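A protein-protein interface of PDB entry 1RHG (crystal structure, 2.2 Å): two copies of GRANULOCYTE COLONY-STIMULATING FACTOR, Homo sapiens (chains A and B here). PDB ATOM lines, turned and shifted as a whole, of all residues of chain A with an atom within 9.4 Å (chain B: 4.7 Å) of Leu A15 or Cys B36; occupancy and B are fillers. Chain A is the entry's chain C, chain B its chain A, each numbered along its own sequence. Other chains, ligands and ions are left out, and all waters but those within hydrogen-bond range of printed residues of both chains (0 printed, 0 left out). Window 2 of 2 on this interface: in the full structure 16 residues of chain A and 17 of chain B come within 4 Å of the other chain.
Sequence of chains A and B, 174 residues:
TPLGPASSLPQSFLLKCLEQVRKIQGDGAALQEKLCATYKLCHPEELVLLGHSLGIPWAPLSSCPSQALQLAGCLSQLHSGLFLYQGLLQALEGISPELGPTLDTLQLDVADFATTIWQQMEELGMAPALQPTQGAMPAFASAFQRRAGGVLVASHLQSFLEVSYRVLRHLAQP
No position is printed for both chains.
OE1 of Gln A11 touches O of Cys B42, 3.5 Å away.
Ala B37 touches Ser A12 (CB to OG, 3.8 Å).
Leu A15 touches Glu B33.
Leu A15 touches Cys B36 (CD1 to CB, 3.3 Å).
Of the 20 printed residues of chain A, 4 touch a printed residue of chain B.
Printed residues of chain A that touch a printed residue of chain B: Gln A11, Ser A12, Leu A15 and Glu A19.
Of the 11 printed residues of chain B, 4 touch a printed residue of chain A.
Hydrophobic or aromatic side chains of chain B within 4 Å of the printed part of chain A: Ala B37.
Among the printed residues, 5 pairs touch across the chains.
Among the printed residues, no Asp or Glu carboxylate lies within 4 Å of a Lys or Arg side-chain nitrogen of the other chain.
Leu A15 touches two residues of chain B.
Of chain A, only Leu A15 (3.3 Å) comes within 4 Å of Cys B36.
Ala B37 touches one residue of chain A.
Printed residues of chain B within 4 Å of Glu A19: Glu B33 (2.8 Å).
Of the printed residues of chain B, Ser A12 touches Ala B37 (3.8 Å).
The side-chain sulfur (SG) of Cys B36 forms a disulfide with the side-chain sulfur (SG) of Cys B42.
N of Cys B36 lies close to O of Leu B41, 3.2 Å away.
The side-chain carboxylate (OE2) of Glu B33 lies close to the side-chain carboxylate (OE1) of Glu A19, at 2.8 Å.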
ATOM      1  N   LEU A   9      24.781 -11.503 -20.758  1.00  0.00           N
ATOM      2  CA  LEU A   9      24.027 -10.832 -19.710  1.00  0.00           C
ATOM      3  C   LEU A   9      24.819 -11.008 -18.404  1.00  0.00           C
ATOM      4  O   LEU A   9      25.805 -11.766 -18.455  1.00  0.00           O
ATOM      5  CB  LEU A   9      22.679 -11.500 -19.644  1.00  0.00           C
ATOM      6  CG  LEU A   9      21.772 -11.181 -20.776  1.00  0.00           C
ATOM      7  CD1 LEU A   9      21.246 -12.461 -21.458  1.00  0.00           C
ATOM      8  CD2 LEU A   9      20.756 -10.222 -20.187  1.00  0.00           C
ATOM      9  N   PRO A  10      24.483 -10.399 -17.247  1.00  0.00           N
ATOM     10  CA  PRO A  10      25.037 -10.794 -15.943  1.00  0.00           C
ATOM     11  C   PRO A  10      24.775 -12.279 -15.641  1.00  0.00           C
ATOM     12  O   PRO A  10      23.625 -12.753 -15.594  1.00  0.00           O
ATOM     13  CB  PRO A  10      24.375  -9.854 -14.923  1.00  0.00           C
ATOM     14  CG  PRO A  10      23.057  -9.497 -15.581  1.00  0.00           C
ATOM     15  CD  PRO A  10      23.442  -9.372 -17.067  1.00  0.00           C
ATOM     16  N   GLN A  11      25.881 -13.014 -15.423  1.00  0.00           N
ATOM     17  CA  GLN A  11      25.874 -14.434 -15.079  1.00  0.00           C
ATOM     18  C   GLN A  11      24.979 -14.687 -13.896  1.00  0.00           C
ATOM     19  O   GLN A  11      24.288 -15.690 -13.937  1.00  0.00           O
ATOM     20  CB  GLN A  11      27.248 -14.930 -14.720  1.00  0.00           C
ATOM     21  CG  GLN A  11      27.345 -16.447 -14.834  1.00  0.00           C
ATOM     22  CD  GLN A  11      27.609 -16.978 -16.244  1.00  0.00           C
ATOM     23  OE1 GLN A  11      27.841 -18.173 -16.435  1.00  0.00           O
ATOM     24  NE2 GLN A  11      27.706 -16.160 -17.304  1.00  0.00           N
ATOM     25  N   SER A  12      24.901 -13.823 -12.879  1.00  0.00           N
ATOM     26  CA  SER A  12      23.963 -14.113 -11.822  1.00  0.00           C
ATOM     27  C   SER A  12      22.531 -14.037 -12.335  1.00  0.00           C
ATOM     28  O   SER A  12      21.778 -14.891 -11.858  1.00  0.00           O
ATOM     29  CB  SER A  12      24.035 -13.168 -10.643  1.00  0.00           C
ATOM     30  OG  SER A  12      23.392 -13.756  -9.487  1.00  0.00           O
ATOM     31  N   PHE A  13      22.077 -13.161 -13.263  1.00  0.00           N
ATOM     32  CA  PHE A  13      20.688 -13.196 -13.750  1.00  0.00           C
ATOM     33  C   PHE A  13      20.527 -14.528 -14.450  1.00  0.00           C
ATOM     34  O   PHE A  13      19.480 -15.152 -14.350  1.00  0.00           O
ATOM     35  CB  PHE A  13      20.377 -12.071 -14.780  1.00  0.00           C
ATOM     36  CG  PHE A  13      19.223 -12.261 -15.764  1.00  0.00           C
ATOM     37  CD1 PHE A  13      17.954 -11.836 -15.433  1.00  0.00           C
ATOM     38  CD2 PHE A  13      19.445 -12.819 -17.011  1.00  0.00           C
ATOM     39  CE1 PHE A  13      16.909 -11.958 -16.343  1.00  0.00           C
ATOM     40  CE2 PHE A  13      18.395 -12.939 -17.917  1.00  0.00           C
ATOM     41  CZ  PHE A  13      17.124 -12.508 -17.588  1.00  0.00           C
ATOM     42  N   LEU A  14      21.571 -14.972 -15.123  1.00  0.00           N
ATOM     43  CA  LEU A  14      21.487 -16.194 -15.859  1.00  0.00           C
ATOM     44  C   LEU A  14      21.262 -17.418 -14.998  1.00  0.00           C
ATOM     45  O   LEU A  14      20.525 -18.351 -15.376  1.00  0.00           O
ATOM     46  CB  LEU A  14      22.746 -16.345 -16.629  1.00  0.00           C
ATOM     47  CG  LEU A  14      22.536 -16.574 -18.090  1.00  0.00           C
ATOM     48  CD1 LEU A  14      23.390 -15.541 -18.827  1.00  0.00           C
ATOM     49  CD2 LEU A  14      22.694 -18.084 -18.376  1.00  0.00           C
ATOM     50  N   LEU A  15      21.883 -17.354 -13.811  1.00  0.00           N
ATOM     51  CA  LEU A  15      21.800 -18.442 -12.883  1.00  0.00           C
ATOM     52  C   LEU A  15      20.470 -18.383 -12.202  1.00  0.00           C
ATOM     53  O   LEU A  15      19.897 -19.465 -12.060  1.00  0.00           O
ATOM     54  CB  LEU A  15      22.994 -18.335 -11.924  1.00  0.00           C
ATOM     55  CG  LEU A  15      24.352 -18.644 -12.621  1.00  0.00           C
ATOM     56  CD1 LEU A  15      25.463 -18.421 -11.637  1.00  0.00           C
ATOM     57  CD2 LEU A  15      24.343 -20.074 -13.219  1.00  0.00           C
ATOM     58  N   LYS A  16      19.935 -17.215 -11.841  1.00  0.00           N
ATOM     59  CA  LYS A  16      18.523 -17.079 -11.409  1.00  0.00           C
ATOM     60  C   LYS A  16      17.544 -17.629 -12.457  1.00  0.00           C
ATOM     61  O   LYS A  16      16.626 -18.384 -12.158  1.00  0.00           O
ATOM     62  CB  LYS A  16      18.076 -15.632 -11.204  1.00  0.00           C
ATOM     63  N   CYS A  17      17.702 -17.366 -13.736  1.00  0.00           N
ATOM     64  CA  CYS A  17      16.832 -17.968 -14.722  1.00  0.00           C
ATOM     65  C   CYS A  17      16.970 -19.462 -14.779  1.00  0.00           C
ATOM     66  O   CYS A  17      15.928 -20.130 -14.728  1.00  0.00           O
ATOM     67  CB  CYS A  17      17.103 -17.497 -16.114  1.00  0.00           C
ATOM     68  SG  CYS A  17      16.767 -15.745 -16.221  1.00  0.00           S
ATOM     69  N   LEU A  18      18.190 -20.033 -14.873  1.00  0.00           N
ATOM     70  CA  LEU A  18      18.348 -21.486 -15.043  1.00  0.00           C
ATOM     71  C   LEU A  18      17.711 -22.218 -13.885  1.00  0.00           C
ATOM     72  O   LEU A  18      17.095 -23.243 -14.044  1.00  0.00           O
ATOM     73  CB  LEU A  18      19.850 -21.797 -15.203  1.00  0.00           C
ATOM     74  CG  LEU A  18      20.502 -21.153 -16.499  1.00  0.00           C
ATOM     75  CD1 LEU A  18      22.001 -21.113 -16.363  1.00  0.00           C
ATOM     76  CD2 LEU A  18      20.176 -21.956 -17.769  1.00  0.00           C
ATOM     77  N   GLU A  19      17.691 -21.625 -12.718  1.00  0.00           N
ATOM     78  CA  GLU A  19      16.965 -22.121 -11.579  1.00  0.00           C
ATOM     79  C   GLU A  19      15.449 -22.123 -11.796  1.00  0.00           C
ATOM     80  O   GLU A  19      14.813 -23.142 -11.513  1.00  0.00           O
ATOM     81  CB  GLU A  19      17.329 -21.229 -10.434  1.00  0.00           C
ATOM     82  CG  GLU A  19      16.935 -21.760  -9.099  1.00  0.00           C
ATOM     83  CD  GLU A  19      16.961 -20.729  -7.975  1.00  0.00           C
ATOM     84  OE1 GLU A  19      17.554 -19.618  -8.093  1.00  0.00           O
ATOM     85  OE2 GLU A  19      16.330 -21.100  -6.971  1.00  0.00           O
ATOM     86  N   GLN A  20      14.844 -20.989 -12.203  1.00  0.00           N
ATOM     87  CA  GLN A  20      13.416 -20.876 -12.470  1.00  0.00           C
ATOM     88  C   GLN A  20      13.010 -21.769 -13.639  1.00  0.00           C
ATOM     89  O   GLN A  20      11.930 -22.366 -13.563  1.00  0.00           O
ATOM     90  CB  GLN A  20      13.021 -19.441 -12.786  1.00  0.00           C
ATOM     91  CG  GLN A  20      12.859 -18.543 -11.573  1.00  0.00           C
ATOM     92  CD  GLN A  20      12.653 -17.078 -11.970  1.00  0.00           C
ATOM     93  OE1 GLN A  20      13.254 -16.605 -12.934  1.00  0.00           O
ATOM     94  NE2 GLN A  20      11.830 -16.237 -11.346  1.00  0.00           N
ATOM     95  N   VAL A  21      13.794 -21.997 -14.687  1.00  0.00           N
ATOM     96  CA  VAL A  21      13.435 -22.982 -15.686  1.00  0.00           C
ATOM     97  C   VAL A  21      13.181 -24.316 -14.981  1.00  0.00           C
ATOM     98  O   VAL A  21      12.080 -24.863 -15.056  1.00  0.00           O
ATOM     99  CB  VAL A  21      14.586 -23.113 -16.685  1.00  0.00           C
ATOM    100  CG1 VAL A  21      14.419 -24.277 -17.621  1.00  0.00           C
ATOM    101  CG2 VAL A  21      14.612 -21.842 -17.502  1.00  0.00           C
ATOM    102  N   ARG A  22      14.111 -24.805 -14.134  1.00  0.00           N
ATOM    103  CA  ARG A  22      13.980 -26.120 -13.511  1.00  0.00           C
ATOM    104  C   ARG A  22      12.816 -26.113 -12.585  1.00  0.00           C
ATOM    105  O   ARG A  22      12.074 -27.066 -12.598  1.00  0.00           O
ATOM    106  CB  ARG A  22      15.209 -26.540 -12.711  1.00  0.00           C
ATOM    107  CG  ARG A  22      16.481 -26.698 -13.521  1.00  0.00           C
ATOM    108  CD  ARG A  22      16.309 -27.478 -14.816  1.00  0.00           C
ATOM    109  NE  ARG A  22      17.591 -27.745 -15.441  1.00  0.00           N
ATOM    110  CZ  ARG A  22      17.746 -28.199 -16.686  1.00  0.00           C
ATOM    111  NH1 ARG A  22      16.765 -28.460 -17.554  1.00  0.00           N
ATOM    112  NH2 ARG A  22      18.978 -28.538 -17.035  1.00  0.00           N
ATOM    113  N   LYS A  23      12.528 -25.076 -11.851  1.00  0.00           N
ATOM    114  CA  LYS A  23      11.398 -25.085 -10.941  1.00  0.00           C
ATOM    115  C   LYS A  23      10.131 -25.176 -11.764  1.00  0.00           C
ATOM    116  O   LYS A  23       9.145 -25.724 -11.272  1.00  0.00           O
ATOM    117  CB  LYS A  23      11.383 -23.820 -10.137  1.00  0.00           C
ATOM    118  CG  LYS A  23      10.465 -23.915  -8.959  1.00  0.00           C
ATOM    119  CD  LYS A  23      10.294 -22.513  -8.368  1.00  0.00           C
ATOM    120  CE  LYS A  23      11.568 -21.795  -7.869  1.00  0.00           C
ATOM    121  NZ  LYS A  23      11.326 -20.361  -7.747  1.00  0.00           N
ATOM    122  N   PHE A 113       8.837 -16.172 -13.534  1.00  0.00           N
ATOM    123  CA  PHE A 113       9.919 -16.246 -14.470  1.00  0.00           C
ATOM    124  C   PHE A 113       9.766 -15.100 -15.497  1.00  0.00           C
ATOM    125  O   PHE A 113      10.711 -14.338 -15.789  1.00  0.00           O
ATOM    126  CB  PHE A 113       9.864 -17.610 -15.145  1.00  0.00           C
ATOM    127  CG  PHE A 113      11.100 -17.858 -16.002  1.00  0.00           C
ATOM    128  CD1 PHE A 113      12.287 -17.152 -15.787  1.00  0.00           C
ATOM    129  CD2 PHE A 113      11.009 -18.798 -17.014  1.00  0.00           C
ATOM    130  CE1 PHE A 113      13.362 -17.408 -16.604  1.00  0.00           C
ATOM    131  CE2 PHE A 113      12.097 -19.040 -17.815  1.00  0.00           C
ATOM    132  CZ  PHE A 113      13.269 -18.346 -17.611  1.00  0.00           C
ATOM    133  N   THR A 116      10.738 -11.896 -14.362  1.00  0.00           N
ATOM    134  CA  THR A 116      12.172 -11.755 -14.231  1.00  0.00           C
ATOM    135  C   THR A 116      12.747 -11.312 -15.582  1.00  0.00           C
ATOM    136  O   THR A 116      13.545 -10.364 -15.601  1.00  0.00           O
ATOM    137  CB  THR A 116      12.682 -13.146 -13.698  1.00  0.00           C
ATOM    138  OG1 THR A 116      12.185 -13.226 -12.347  1.00  0.00           O
ATOM    139  CG2 THR A 116      14.193 -13.358 -13.823  1.00  0.00           C
ATOM    140  N   LEU A 168      19.600 -19.957 -23.069  1.00  0.00           N
ATOM    141  CA  LEU A 168      20.109 -19.074 -22.023  1.00  0.00           C
ATOM    142  C   LEU A 168      21.601 -19.328 -21.907  1.00  0.00           C
ATOM    143  O   LEU A 168      22.355 -18.364 -21.981  1.00  0.00           O
ATOM    144  CB  LEU A 168      19.478 -19.329 -20.652  1.00  0.00           C
ATOM    145  CG  LEU A 168      18.044 -18.896 -20.370  1.00  0.00           C
ATOM    146  CD1 LEU A 168      17.702 -19.292 -18.961  1.00  0.00           C
ATOM    147  CD2 LEU A 168      17.871 -17.399 -20.493  1.00  0.00           C
ATOM    148  N   ARG A 169      22.044 -20.598 -21.840  1.00  0.00           N
ATOM    149  CA  ARG A 169      23.458 -20.994 -21.850  1.00  0.00           C
ATOM    150  C   ARG A 169      24.217 -20.223 -22.941  1.00  0.00           C
ATOM    151  O   ARG A 169      25.287 -19.633 -22.783  1.00  0.00           O
ATOM    152  CB  ARG A 169      23.615 -22.506 -22.152  1.00  0.00           C
ATOM    153  CG  ARG A 169      25.106 -22.869 -22.146  1.00  0.00           C
ATOM    154  CD  ARG A 169      25.706 -24.120 -22.828  1.00  0.00           C
ATOM    155  NE  ARG A 169      27.167 -23.944 -22.751  1.00  0.00           N
ATOM    156  CZ  ARG A 169      28.023 -24.778 -22.140  1.00  0.00           C
ATOM    157  NH1 ARG A 169      27.645 -25.904 -21.537  1.00  0.00           N
ATOM    158  NH2 ARG A 169      29.293 -24.401 -22.042  1.00  0.00           N
ATOM    159  N   ALA A 172      24.555 -16.377 -22.589  1.00  0.00           N
ATOM    160  CA  ALA A 172      25.412 -16.060 -21.450  1.00  0.00           C
ATOM    161  C   ALA A 172      26.705 -15.367 -21.852  1.00  0.00           C
ATOM    162  O   ALA A 172      27.014 -14.360 -21.204  1.00  0.00           O
ATOM    163  CB  ALA A 172      25.827 -17.299 -20.674  1.00  0.00           C
ATOM    164  N   GLN B  32      24.385 -23.300  -7.198  1.00  0.00           N
ATOM    165  CA  GLN B  32      25.187 -22.544  -8.129  1.00  0.00           C
ATOM    166  C   GLN B  32      24.951 -21.070  -7.993  1.00  0.00           C
ATOM    167  O   GLN B  32      25.912 -20.312  -7.767  1.00  0.00           O
ATOM    168  CB  GLN B  32      24.900 -22.827  -9.575  1.00  0.00           C
ATOM    169  CG  GLN B  32      25.760 -23.970  -9.906  1.00  0.00           C
ATOM    170  CD  GLN B  32      25.631 -24.500 -11.313  1.00  0.00           C
ATOM    171  OE1 GLN B  32      24.865 -25.398 -11.720  1.00  0.00           O
ATOM    172  NE2 GLN B  32      26.532 -23.918 -12.070  1.00  0.00           N
ATOM    173  N   GLU B  33      23.680 -20.642  -8.004  1.00  0.00           N
ATOM    174  CA  GLU B  33      23.433 -19.216  -8.031  1.00  0.00           C
ATOM    175  C   GLU B  33      23.734 -18.597  -6.699  1.00  0.00           C
ATOM    176  O   GLU B  33      24.073 -17.419  -6.643  1.00  0.00           O
ATOM    177  CB  GLU B  33      21.992 -18.974  -8.482  1.00  0.00           C
ATOM    178  CG  GLU B  33      20.900 -19.085  -7.480  1.00  0.00           C
ATOM    179  CD  GLU B  33      20.386 -17.727  -6.992  1.00  0.00           C
ATOM    180  OE1 GLU B  33      21.193 -16.863  -6.589  1.00  0.00           O
ATOM    181  OE2 GLU B  33      19.151 -17.562  -7.012  1.00  0.00           O
ATOM    182  N   LYS B  34      23.661 -19.335  -5.606  1.00  0.00           N
ATOM    183  CA  LYS B  34      24.087 -18.786  -4.333  1.00  0.00           C
ATOM    184  C   LYS B  34      25.613 -18.738  -4.286  1.00  0.00           C
ATOM    185  O   LYS B  34      26.186 -17.808  -3.701  1.00  0.00           O
ATOM    186  CB  LYS B  34      23.585 -19.637  -3.185  1.00  0.00           C
ATOM    187  CG  LYS B  34      22.133 -19.341  -2.946  1.00  0.00           C
ATOM    188  CD  LYS B  34      21.599 -20.554  -2.220  1.00  0.00           C
ATOM    189  CE  LYS B  34      20.101 -20.460  -2.027  1.00  0.00           C
ATOM    190  NZ  LYS B  34      19.781 -19.456  -1.025  1.00  0.00           N
ATOM    191  N   LEU B  35      26.350 -19.669  -4.879  1.00  0.00           N
ATOM    192  CA  LEU B  35      27.778 -19.567  -4.782  1.00  0.00           C
ATOM    193  C   LEU B  35      28.229 -18.436  -5.699  1.00  0.00           C
ATOM    194  O   LEU B  35      29.057 -17.587  -5.328  1.00  0.00           O
ATOM    195  CB  LEU B  35      28.400 -20.892  -5.181  1.00  0.00           C
ATOM    196  CG  LEU B  35      28.217 -22.101  -4.297  1.00  0.00           C
ATOM    197  CD1 LEU B  35      28.919 -23.247  -4.940  1.00  0.00           C
ATOM    198  CD2 LEU B  35      28.775 -21.860  -2.924  1.00  0.00           C
ATOM    199  N   CYS B  36      27.620 -18.336  -6.872  1.00  0.00           N
ATOM    200  CA  CYS B  36      27.959 -17.299  -7.796  1.00  0.00           C
ATOM    201  C   CYS B  36      27.632 -15.979  -7.235  1.00  0.00           C
ATOM    202  O   CYS B  36      28.393 -15.058  -7.466  1.00  0.00           O
ATOM    203  CB  CYS B  36      27.219 -17.388  -9.067  1.00  0.00           C
ATOM    204  SG  CYS B  36      27.244 -15.805  -9.952  1.00  0.00           S
ATOM    205  N   ALA B  37      26.563 -15.882  -6.475  1.00  0.00           N
ATOM    206  CA  ALA B  37      26.196 -14.597  -5.943  1.00  0.00           C
ATOM    207  C   ALA B  37      26.713 -14.356  -4.537  1.00  0.00           C
ATOM    208  O   ALA B  37      26.636 -13.220  -4.100  1.00  0.00           O
ATOM    209  CB  ALA B  37      24.652 -14.484  -6.013  1.00  0.00           C
ATOM    210  N   THR B  38      27.231 -15.306  -3.751  1.00  0.00           N
ATOM    211  CA  THR B  38      27.793 -14.999  -2.429  1.00  0.00           C
ATOM    212  C   THR B  38      29.301 -14.772  -2.561  1.00  0.00           C
ATOM    213  O   THR B  38      29.930 -13.904  -1.955  1.00  0.00           O
ATOM    214  CB  THR B  38      27.563 -16.151  -1.421  1.00  0.00           C
ATOM    215  OG1 THR B  38      26.163 -16.360  -1.295  1.00  0.00           O
ATOM    216  CG2 THR B  38      28.118 -15.823  -0.054  1.00  0.00           C
ATOM    217  N   TYR B  39      29.912 -15.598  -3.396  1.00  0.00           N
ATOM    218  CA  TYR B  39      31.345 -15.564  -3.560  1.00  0.00           C
ATOM    219  C   TYR B  39      31.763 -15.465  -5.016  1.00  0.00           C
ATOM    220  O   TYR B  39      32.771 -16.030  -5.423  1.00  0.00           O
ATOM    221  CB  TYR B  39      31.981 -16.804  -2.978  1.00  0.00           C
ATOM    222  CG  TYR B  39      31.365 -17.336  -1.717  1.00  0.00           C
ATOM    223  CD1 TYR B  39      31.628 -16.779  -0.485  1.00  0.00           C
ATOM    224  CD2 TYR B  39      30.591 -18.463  -1.857  1.00  0.00           C
ATOM    225  CE1 TYR B  39      31.110 -17.400   0.632  1.00  0.00           C
ATOM    226  CE2 TYR B  39      30.073 -19.077  -0.748  1.00  0.00           C
ATOM    227  CZ  TYR B  39      30.348 -18.545   0.489  1.00  0.00           C
ATOM    228  OH  TYR B  39      29.890 -19.245   1.594  1.00  0.00           O
ATOM    229  N   LYS B  40      30.957 -14.845  -5.848  1.00  0.00           N
ATOM    230  CA  LYS B  40      31.342 -14.483  -7.189  1.00  0.00           C
ATOM    231  C   LYS B  40      32.009 -15.581  -7.983  1.00  0.00           C
ATOM    232  O   LYS B  40      32.768 -15.286  -8.925  1.00  0.00           O
ATOM    233  CB  LYS B  40      32.228 -13.202  -7.086  1.00  0.00           C
ATOM    234  CG  LYS B  40      31.508 -11.964  -6.511  1.00  0.00           C
ATOM    235  CD  LYS B  40      32.512 -10.928  -5.975  1.00  0.00           C
ATOM    236  CE  LYS B  40      31.934  -9.508  -5.639  1.00  0.00           C
ATOM    237  NZ  LYS B  40      32.906  -8.541  -5.099  1.00  0.00           N
ATOM    238  N   LEU B  41      31.714 -16.853  -7.613  1.00  0.00           N
ATOM    239  CA  LEU B  41      32.222 -18.024  -8.351  1.00  0.00           C
ATOM    240  C   LEU B  41      31.038 -18.376  -9.210  1.00  0.00           C
ATOM    241  O   LEU B  41      30.069 -18.988  -8.757  1.00  0.00           O
ATOM    242  CB  LEU B  41      32.564 -19.215  -7.449  1.00  0.00           C
ATOM    243  CG  LEU B  41      33.739 -18.948  -6.532  1.00  0.00           C
ATOM    244  CD1 LEU B  41      33.360 -19.427  -5.177  1.00  0.00           C
ATOM    245  CD2 LEU B  41      34.999 -19.580  -7.064  1.00  0.00           C
ATOM    246  N   CYS B  42      31.094 -17.848 -10.429  1.00  0.00           N
ATOM    247  CA  CYS B  42      29.995 -17.960 -11.344  1.00  0.00           C
ATOM    248  C   CYS B  42      30.431 -18.729 -12.537  1.00  0.00           C
ATOM    249  O   CYS B  42      29.705 -18.810 -13.507  1.00  0.00           O
ATOM    250  CB  CYS B  42      29.518 -16.548 -11.721  1.00  0.00           C
ATOM    251  SG  CYS B  42      29.198 -15.482 -10.266  1.00  0.00           S
